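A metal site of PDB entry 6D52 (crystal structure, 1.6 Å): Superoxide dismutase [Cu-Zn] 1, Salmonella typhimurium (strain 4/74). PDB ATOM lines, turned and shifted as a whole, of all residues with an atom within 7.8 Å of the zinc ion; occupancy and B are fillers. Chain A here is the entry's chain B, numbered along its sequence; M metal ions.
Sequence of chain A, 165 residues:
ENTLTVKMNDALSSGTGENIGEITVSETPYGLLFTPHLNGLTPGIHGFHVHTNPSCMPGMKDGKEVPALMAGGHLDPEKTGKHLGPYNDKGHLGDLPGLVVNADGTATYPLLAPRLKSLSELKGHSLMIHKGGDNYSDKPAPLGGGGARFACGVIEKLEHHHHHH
The zinc ion is bound by OD1 of Asp 95 (1.9 Å), ND1 of His 92 (2.0 Å), ND1 of His 74 (2.0 Å) and ND1 of His 83 (2.1 Å).
The zinc ion has four donor atoms within binding distance.
N of His 92 sits at hydrogen-bond distance from OG1 of Thr 80.
N of His 92 sits at hydrogen-bond distance from O of Lys 82, 2.8 Å away.
The side-chain carboxylate (OD1) of Asp 134 lies within hydrogen-bond range of a ring nitrogen (NE2) of His 83 (2.8 Å).
OD2 of Asp 95 lies within hydrogen-bond range of N of Leu 84.
O of His 92 lies within hydrogen-bond range of NH1 of Arg 115 (2.9 Å).
N of His 83 is in hydrogen-bond range of OD2 of Asp 138, 2.9 Å away.
A ring nitrogen (ND1) of His 49 sits close to a ring nitrogen (NE2) of His 74 (3.3 Å).
The side-chain carboxylate (OD2) of Asp 95 sits at hydrogen-bond distance from the backbone NH (N) of Gly 85 (3.1 Å).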
ATOM      1  N   PHE A  48     -13.816  27.199 -24.854  1.00  0.00           N
ATOM      2  CA  PHE A  48     -14.686  26.123 -25.333  1.00  0.00           C
ATOM      3  C   PHE A  48     -14.036  24.822 -24.888  1.00  0.00           C
ATOM      4  O   PHE A  48     -12.923  24.513 -25.316  1.00  0.00           O
ATOM      5  CB  PHE A  48     -14.801  26.239 -26.861  1.00  0.00           C
ATOM      6  CG  PHE A  48     -15.635  25.178 -27.529  1.00  0.00           C
ATOM      7  CD1 PHE A  48     -16.881  24.844 -27.046  1.00  0.00           C
ATOM      8  CD2 PHE A  48     -15.205  24.570 -28.713  1.00  0.00           C
ATOM      9  CE1 PHE A  48     -17.650  23.891 -27.677  1.00  0.00           C
ATOM     10  CE2 PHE A  48     -15.970  23.608 -29.346  1.00  0.00           C
ATOM     11  CZ  PHE A  48     -17.216  23.292 -28.832  1.00  0.00           C
ATOM     12  N   HIS A  49     -14.689  24.080 -23.999  1.00  0.00           N
ATOM     13  CA  HIS A  49     -14.077  22.862 -23.463  1.00  0.00           C
ATOM     14  C   HIS A  49     -15.134  21.814 -23.165  1.00  0.00           C
ATOM     15  O   HIS A  49     -16.320  22.120 -22.945  1.00  0.00           O
ATOM     16  CB  HIS A  49     -13.305  23.109 -22.163  1.00  0.00           C
ATOM     17  CG  HIS A  49     -12.758  24.497 -22.020  1.00  0.00           C
ATOM     18  ND1 HIS A  49     -13.305  25.438 -21.194  1.00  0.00           N
ATOM     19  CD2 HIS A  49     -11.705  25.105 -22.625  1.00  0.00           C
ATOM     20  CE1 HIS A  49     -12.608  26.551 -21.240  1.00  0.00           C
ATOM     21  NE2 HIS A  49     -11.633  26.371 -22.120  1.00  0.00           N
ATOM     22  N   VAL A  50     -14.685  20.564 -23.172  1.00  0.00           N
ATOM     23  CA  VAL A  50     -15.475  19.463 -22.636  1.00  0.00           C
ATOM     24  C   VAL A  50     -15.296  19.441 -21.136  1.00  0.00           C
ATOM     25  O   VAL A  50     -14.158  19.430 -20.639  1.00  0.00           O
ATOM     26  CB  VAL A  50     -15.062  18.121 -23.256  1.00  0.00           C
ATOM     27  CG1 VAL A  50     -16.094  17.037 -22.849  1.00  0.00           C
ATOM     28  CG2 VAL A  50     -14.923  18.192 -24.753  1.00  0.00           C
ATOM     29  N   HIS A  51     -16.401  19.415 -20.411  1.00  0.00           N
ATOM     30  CA  HIS A  51     -16.396  19.318 -18.949  1.00  0.00           C
ATOM     31  C   HIS A  51     -16.889  17.937 -18.522  1.00  0.00           C
ATOM     32  O   HIS A  51     -17.545  17.217 -19.286  1.00  0.00           O
ATOM     33  CB  HIS A  51     -17.244  20.412 -18.322  1.00  0.00           C
ATOM     34  CG  HIS A  51     -16.617  21.768 -18.361  1.00  0.00           C
ATOM     35  ND1 HIS A  51     -16.410  22.526 -17.237  1.00  0.00           N
ATOM     36  CD2 HIS A  51     -16.114  22.489 -19.388  1.00  0.00           C
ATOM     37  CE1 HIS A  51     -15.850  23.673 -17.562  1.00  0.00           C
ATOM     38  NE2 HIS A  51     -15.642  23.673 -18.867  1.00  0.00           N
ATOM     39  N   GLY A  73     -15.416  20.360 -13.756  1.00  0.00           N
ATOM     40  CA  GLY A  73     -14.257  20.977 -14.358  1.00  0.00           C
ATOM     41  C   GLY A  73     -13.990  20.470 -15.754  1.00  0.00           C
ATOM     42  O   GLY A  73     -14.755  19.719 -16.338  1.00  0.00           O
ATOM     43  N   HIS A  74     -12.845  20.878 -16.291  1.00  0.00           N
ATOM     44  CA  HIS A  74     -12.430  20.399 -17.607  1.00  0.00           C
ATOM     45  C   HIS A  74     -12.143  18.898 -17.587  1.00  0.00           C
ATOM     46  O   HIS A  74     -11.496  18.373 -16.666  1.00  0.00           O
ATOM     47  CB  HIS A  74     -11.183  21.134 -18.097  1.00  0.00           C
ATOM     48  CG  HIS A  74     -11.371  22.604 -18.252  1.00  0.00           C
ATOM     49  ND1 HIS A  74     -10.472  23.407 -18.924  1.00  0.00           N
ATOM     50  CD2 HIS A  74     -12.370  23.436 -17.833  1.00  0.00           C
ATOM     51  CE1 HIS A  74     -10.893  24.655 -18.902  1.00  0.00           C
ATOM     52  NE2 HIS A  74     -12.033  24.698 -18.232  1.00  0.00           N
ATOM     53  N   LEU A  75     -12.634  18.199 -18.610  1.00  0.00           N
ATOM     54  CA  LEU A  75     -12.414  16.776 -18.732  1.00  0.00           C
ATOM     55  C   LEU A  75     -10.920  16.475 -18.708  1.00  0.00           C
ATOM     56  O   LEU A  75     -10.139  17.059 -19.472  1.00  0.00           O
ATOM     57  CB  LEU A  75     -13.050  16.256 -20.013  1.00  0.00           C
ATOM     58  CG  LEU A  75     -12.853  14.787 -20.378  1.00  0.00           C
ATOM     59  CD1 LEU A  75     -13.569  13.857 -19.397  1.00  0.00           C
ATOM     60  CD2 LEU A  75     -13.336  14.550 -21.801  1.00  0.00           C
ATOM     61  N   ASP A  76     -10.505  15.570 -17.818  1.00  0.00           N
ATOM     62  CA  ASP A  76      -9.082  15.362 -17.527  1.00  0.00           C
ATOM     63  C   ASP A  76      -8.841  13.923 -17.093  1.00  0.00           C
ATOM     64  O   ASP A  76      -8.410  13.676 -15.959  1.00  0.00           O
ATOM     65  CB  ASP A  76      -8.647  16.356 -16.447  1.00  0.00           C
ATOM     66  CG  ASP A  76      -7.130  16.473 -16.303  1.00  0.00           C
ATOM     67  OD1 ASP A  76      -6.373  16.090 -17.206  1.00  0.00           O
ATOM     68  OD2 ASP A  76      -6.708  16.988 -15.238  1.00  0.00           O
ATOM     69  N   THR A  80      -3.991  15.462 -15.391  1.00  0.00           N
ATOM     70  CA  THR A  80      -2.876  16.370 -15.597  1.00  0.00           C
ATOM     71  C   THR A  80      -2.939  17.564 -14.666  1.00  0.00           C
ATOM     72  O   THR A  80      -1.899  18.100 -14.264  1.00  0.00           O
ATOM     73  CB  THR A  80      -2.853  16.855 -17.042  1.00  0.00           C
ATOM     74  OG1 THR A  80      -3.969  17.729 -17.271  1.00  0.00           O
ATOM     75  CG2 THR A  80      -2.916  15.692 -18.021  1.00  0.00           C
ATOM     76  N   GLY A  81      -4.150  18.031 -14.334  1.00  0.00           N
ATOM     77  CA  GLY A  81      -4.299  19.243 -13.564  1.00  0.00           C
ATOM     78  C   GLY A  81      -3.778  20.501 -14.220  1.00  0.00           C
ATOM     79  O   GLY A  81      -3.504  21.489 -13.530  1.00  0.00           O
ATOM     80  N   LYS A  82      -3.642  20.508 -15.550  1.00  0.00           N
ATOM     81  CA  LYS A  82      -3.080  21.638 -16.263  1.00  0.00           C
ATOM     82  C   LYS A  82      -3.945  21.960 -17.470  1.00  0.00           C
ATOM     83  O   LYS A  82      -4.363  21.049 -18.202  1.00  0.00           O
ATOM     84  CB  LYS A  82      -1.643  21.362 -16.727  1.00  0.00           C
ATOM     85  CG  LYS A  82      -0.666  21.177 -15.567  1.00  0.00           C
ATOM     86  CD  LYS A  82       0.767  21.406 -16.005  1.00  0.00           C
ATOM     87  CE  LYS A  82       1.373  20.180 -16.597  1.00  0.00           C
ATOM     88  NZ  LYS A  82       2.363  19.582 -15.653  1.00  0.00           N
ATOM     89  N   HIS A  83      -4.151  23.238 -17.711  1.00  0.00           N
ATOM     90  CA  HIS A  83      -4.878  23.718 -18.883  1.00  0.00           C
ATOM     91  C   HIS A  83      -3.877  24.154 -19.945  1.00  0.00           C
ATOM     92  O   HIS A  83      -3.265  25.225 -19.826  1.00  0.00           O
ATOM     93  CB  HIS A  83      -5.821  24.859 -18.508  1.00  0.00           C
ATOM     94  CG  HIS A  83      -6.618  25.364 -19.662  1.00  0.00           C
ATOM     95  ND1 HIS A  83      -7.758  24.731 -20.129  1.00  0.00           N
ATOM     96  CD2 HIS A  83      -6.414  26.420 -20.491  1.00  0.00           C
ATOM     97  CE1 HIS A  83      -8.208  25.383 -21.184  1.00  0.00           C
ATOM     98  NE2 HIS A  83      -7.408  26.399 -21.433  1.00  0.00           N
ATOM     99  N   LEU A  84      -3.723  23.333 -20.985  1.00  0.00           N
ATOM    100  CA  LEU A  84      -2.735  23.631 -22.018  1.00  0.00           C
ATOM    101  C   LEU A  84      -3.292  23.624 -23.440  1.00  0.00           C
ATOM    102  O   LEU A  84      -2.515  23.720 -24.395  1.00  0.00           O
ATOM    103  CB  LEU A  84      -1.561  22.643 -21.915  1.00  0.00           C
ATOM    104  CG  LEU A  84      -0.651  22.935 -20.714  1.00  0.00           C
ATOM    105  CD1 LEU A  84       0.264  21.781 -20.441  1.00  0.00           C
ATOM    106  CD2 LEU A  84       0.166  24.215 -20.947  1.00  0.00           C
ATOM    107  N   GLY A  85      -4.618  23.542 -23.608  1.00  0.00           N
ATOM    108  CA  GLY A  85      -5.213  23.691 -24.914  1.00  0.00           C
ATOM    109  C   GLY A  85      -5.253  22.423 -25.748  1.00  0.00           C
ATOM    110  O   GLY A  85      -4.862  21.335 -25.315  1.00  0.00           O
ATOM    111  N   GLY A  91      -1.976  18.544 -20.947  1.00  0.00           N
ATOM    112  CA  GLY A  91      -3.070  19.186 -20.239  1.00  0.00           C
ATOM    113  C   GLY A  91      -4.408  18.486 -20.432  1.00  0.00           C
ATOM    114  O   GLY A  91      -4.473  17.407 -21.037  1.00  0.00           O
ATOM    115  N   HIS A  92      -5.483  19.115 -19.933  1.00  0.00           N
ATOM    116  CA  HIS A  92      -6.815  18.529 -19.966  1.00  0.00           C
ATOM    117  C   HIS A  92      -7.179  18.031 -21.351  1.00  0.00           C
ATOM    118  O   HIS A  92      -7.127  18.795 -22.316  1.00  0.00           O
ATOM    119  CB  HIS A  92      -7.872  19.557 -19.572  1.00  0.00           C
ATOM    120  CG  HIS A  92      -7.589  20.319 -18.321  1.00  0.00           C
ATOM    121  ND1 HIS A  92      -7.749  21.686 -18.245  1.00  0.00           N
ATOM    122  CD2 HIS A  92      -7.234  19.900 -17.085  1.00  0.00           C
ATOM    123  CE1 HIS A  92      -7.489  22.084 -17.011  1.00  0.00           C
ATOM    124  NE2 HIS A  92      -7.164  21.022 -16.283  1.00  0.00           N
ATOM    125  N   LEU A  93      -7.643  16.777 -21.438  1.00  0.00           N
ATOM    126  CA  LEU A  93      -8.126  16.239 -22.700  1.00  0.00           C
ATOM    127  C   LEU A  93      -9.328  17.005 -23.216  1.00  0.00           C
ATOM    128  O   LEU A  93      -9.570  17.043 -24.423  1.00  0.00           O
ATOM    129  CB  LEU A  93      -8.480  14.750 -22.542  1.00  0.00           C
ATOM    130  CG  LEU A  93      -9.010  14.028 -23.774  1.00  0.00           C
ATOM    131  CD1 LEU A  93      -7.986  14.070 -24.909  1.00  0.00           C
ATOM    132  CD2 LEU A  93      -9.391  12.584 -23.449  1.00  0.00           C
ATOM    133  N   GLY A  94     -10.109  17.607 -22.324  1.00  0.00           N
ATOM    134  CA  GLY A  94     -11.286  18.329 -22.745  1.00  0.00           C
ATOM    135  C   GLY A  94     -11.048  19.695 -23.343  1.00  0.00           C
ATOM    136  O   GLY A  94     -12.009  20.365 -23.709  1.00  0.00           O
ATOM    137  N   ASP A  95      -9.783  20.121 -23.450  1.00  0.00           N
ATOM    138  CA  ASP A  95      -9.449  21.451 -23.971  1.00  0.00           C
ATOM    139  C   ASP A  95      -9.626  21.497 -25.485  1.00  0.00           C
ATOM    140  O   ASP A  95      -8.870  20.868 -26.233  1.00  0.00           O
ATOM    141  CB  ASP A  95      -8.011  21.821 -23.583  1.00  0.00           C
ATOM    142  CG  ASP A  95      -7.851  22.108 -22.108  1.00  0.00           C
ATOM    143  OD1 ASP A  95      -8.883  22.175 -21.370  1.00  0.00           O
ATOM    144  OD2 ASP A  95      -6.693  22.266 -21.685  1.00  0.00           O
ATOM    145  N   LEU A  96     -10.628  22.228 -25.950  1.00  0.00           N
ATOM    146  CA  LEU A  96     -10.890  22.381 -27.368  1.00  0.00           C
ATOM    147  C   LEU A  96     -10.349  23.703 -27.860  1.00  0.00           C
ATOM    148  O   LEU A  96     -10.036  24.597 -27.073  1.00  0.00           O
ATOM    149  CB  LEU A  96     -12.397  22.291 -27.615  1.00  0.00           C
ATOM    150  CG  LEU A  96     -13.086  21.091 -26.997  1.00  0.00           C
ATOM    151  CD1 LEU A  96     -14.579  21.152 -27.281  1.00  0.00           C
ATOM    152  CD2 LEU A  96     -12.501  19.763 -27.528  1.00  0.00           C
ATOM    153  N   ARG A 115      -6.707  15.834 -30.449  1.00  0.00           N
ATOM    154  CA  ARG A 115      -6.425  14.868 -29.403  1.00  0.00           C
ATOM    155  C   ARG A 115      -7.594  13.949 -29.112  1.00  0.00           C
ATOM    156  O   ARG A 115      -7.399  12.892 -28.491  1.00  0.00           O
ATOM    157  CB  ARG A 115      -6.028  15.584 -28.116  1.00  0.00           C
ATOM    158  CG  ARG A 115      -4.752  16.393 -28.219  1.00  0.00           C
ATOM    159  CD  ARG A 115      -4.603  17.329 -27.055  1.00  0.00           C
ATOM    160  NE  ARG A 115      -4.565  16.589 -25.805  1.00  0.00           N
ATOM    161  CZ  ARG A 115      -4.846  17.092 -24.609  1.00  0.00           C
ATOM    162  NH1 ARG A 115      -5.206  18.372 -24.471  1.00  0.00           N
ATOM    163  NH2 ARG A 115      -4.773  16.303 -23.559  1.00  0.00           N
ATOM    164  N   ASP A 134      -9.569  32.021 -24.462  1.00  0.00           N
ATOM    165  CA  ASP A 134      -8.719  30.903 -24.071  1.00  0.00           C
ATOM    166  C   ASP A 134      -7.352  31.065 -24.712  1.00  0.00           C
ATOM    167  O   ASP A 134      -7.222  30.926 -25.928  1.00  0.00           O
ATOM    168  CB  ASP A 134      -9.367  29.582 -24.485  1.00  0.00           C
ATOM    169  CG  ASP A 134      -8.719  28.377 -23.841  1.00  0.00           C
ATOM    170  OD1 ASP A 134      -7.626  28.531 -23.242  1.00  0.00           O
ATOM    171  OD2 ASP A 134      -9.316  27.271 -23.892  1.00  0.00           O
ATOM    172  N   TYR A 136      -4.948  29.027 -23.888  1.00  0.00           N
ATOM    173  CA  TYR A 136      -4.399  27.666 -23.806  1.00  0.00           C
ATOM    174  C   TYR A 136      -3.311  27.556 -22.737  1.00  0.00           C
ATOM    175  O   TYR A 136      -2.374  26.762 -22.856  1.00  0.00           O
ATOM    176  CB  TYR A 136      -3.867  27.184 -25.165  1.00  0.00           C
ATOM    177  CG  TYR A 136      -4.852  27.292 -26.332  1.00  0.00           C
ATOM    178  CD1 TYR A 136      -6.220  27.236 -26.133  1.00  0.00           C
ATOM    179  CD2 TYR A 136      -4.390  27.438 -27.661  1.00  0.00           C
ATOM    180  CE1 TYR A 136      -7.105  27.316 -27.194  1.00  0.00           C
ATOM    181  CE2 TYR A 136      -5.264  27.521 -28.703  1.00  0.00           C
ATOM    182  CZ  TYR A 136      -6.632  27.483 -28.474  1.00  0.00           C
ATOM    183  OH  TYR A 136      -7.519  27.615 -29.519  1.00  0.00           O
ATOM    184  N   SER A 137      -3.477  28.290 -21.638  1.00  0.00           N
ATOM    185  CA  SER A 137      -2.495  28.280 -20.570  1.00  0.00           C
ATOM    186  C   SER A 137      -3.200  28.623 -19.259  1.00  0.00           C
ATOM    187  O   SER A 137      -4.294  29.198 -19.266  1.00  0.00           O
ATOM    188  CB  SER A 137      -1.371  29.288 -20.857  1.00  0.00           C
ATOM    189  OG  SER A 137      -0.441  29.374 -19.774  1.00  0.00           O
ATOM    190  N   ASP A 138      -2.562  28.266 -18.142  1.00  0.00           N
ATOM    191  CA  ASP A 138      -3.040  28.654 -16.820  1.00  0.00           C
ATOM    192  C   ASP A 138      -2.507  29.999 -16.355  1.00  0.00           C
ATOM    193  O   ASP A 138      -2.783  30.403 -15.214  1.00  0.00           O
ATOM    194  CB  ASP A 138      -2.664  27.587 -15.792  1.00  0.00           C
ATOM    195  CG  ASP A 138      -3.554  26.358 -15.868  1.00  0.00           C
ATOM    196  OD1 ASP A 138      -4.793  26.499 -15.805  1.00  0.00           O
ATOM    197  OD2 ASP A 138      -3.010  25.246 -15.991  1.00  0.00           O
ATOM    198  N   PRO A 142      -6.078  31.407 -14.688  1.00  0.00           N
ATOM    199  CA  PRO A 142      -6.269  29.962 -14.723  1.00  0.00           C
ATOM    200  C   PRO A 142      -7.252  29.565 -15.821  1.00  0.00           C
ATOM    201  O   PRO A 142      -8.124  30.340 -16.222  1.00  0.00           O
ATOM    202  CB  PRO A 142      -6.810  29.635 -13.321  1.00  0.00           C
ATOM    203  CG  PRO A 142      -7.338  30.924 -12.819  1.00  0.00           C
ATOM    204  CD  PRO A 142      -6.475  31.994 -13.396  1.00  0.00           C
ATOM    205  N   LEU A 143      -7.072  28.343 -16.315  1.00  0.00           N
ATOM    206  CA  LEU A 143      -8.017  27.725 -17.253  1.00  0.00           C
ATOM    207  C   LEU A 143      -8.192  28.584 -18.502  1.00  0.00           C
ATOM    208  O   LEU A 143      -9.285  28.674 -19.067  1.00  0.00           O
ATOM    209  CB  LEU A 143      -9.362  27.468 -16.560  1.00  0.00           C
ATOM    210  CG  LEU A 143      -9.277  26.646 -15.288  1.00  0.00           C
ATOM    211  CD1 LEU A 143     -10.646  26.592 -14.563  1.00  0.00           C
ATOM    212  CD2 LEU A 143      -8.793  25.249 -15.576  1.00  0.00           C
ATOM    213  N   GLY A 144      -7.108  29.237 -18.932  1.00  0.00           N
ATOM    214  CA  GLY A 144      -7.106  29.990 -20.155  1.00  0.00           C
ATOM    215  C   GLY A 144      -7.806  31.331 -20.113  1.00  0.00           C
ATOM    216  O   GLY A 144      -7.882  32.008 -21.143  1.00  0.00           O
HETATM  217 ZN    ZN M   1      -8.609  22.927 -19.615  1.00  0.00          ZN
HETATM  218 CU    CU M   2     -14.745  25.132 -19.867  1.00  0.00          CU
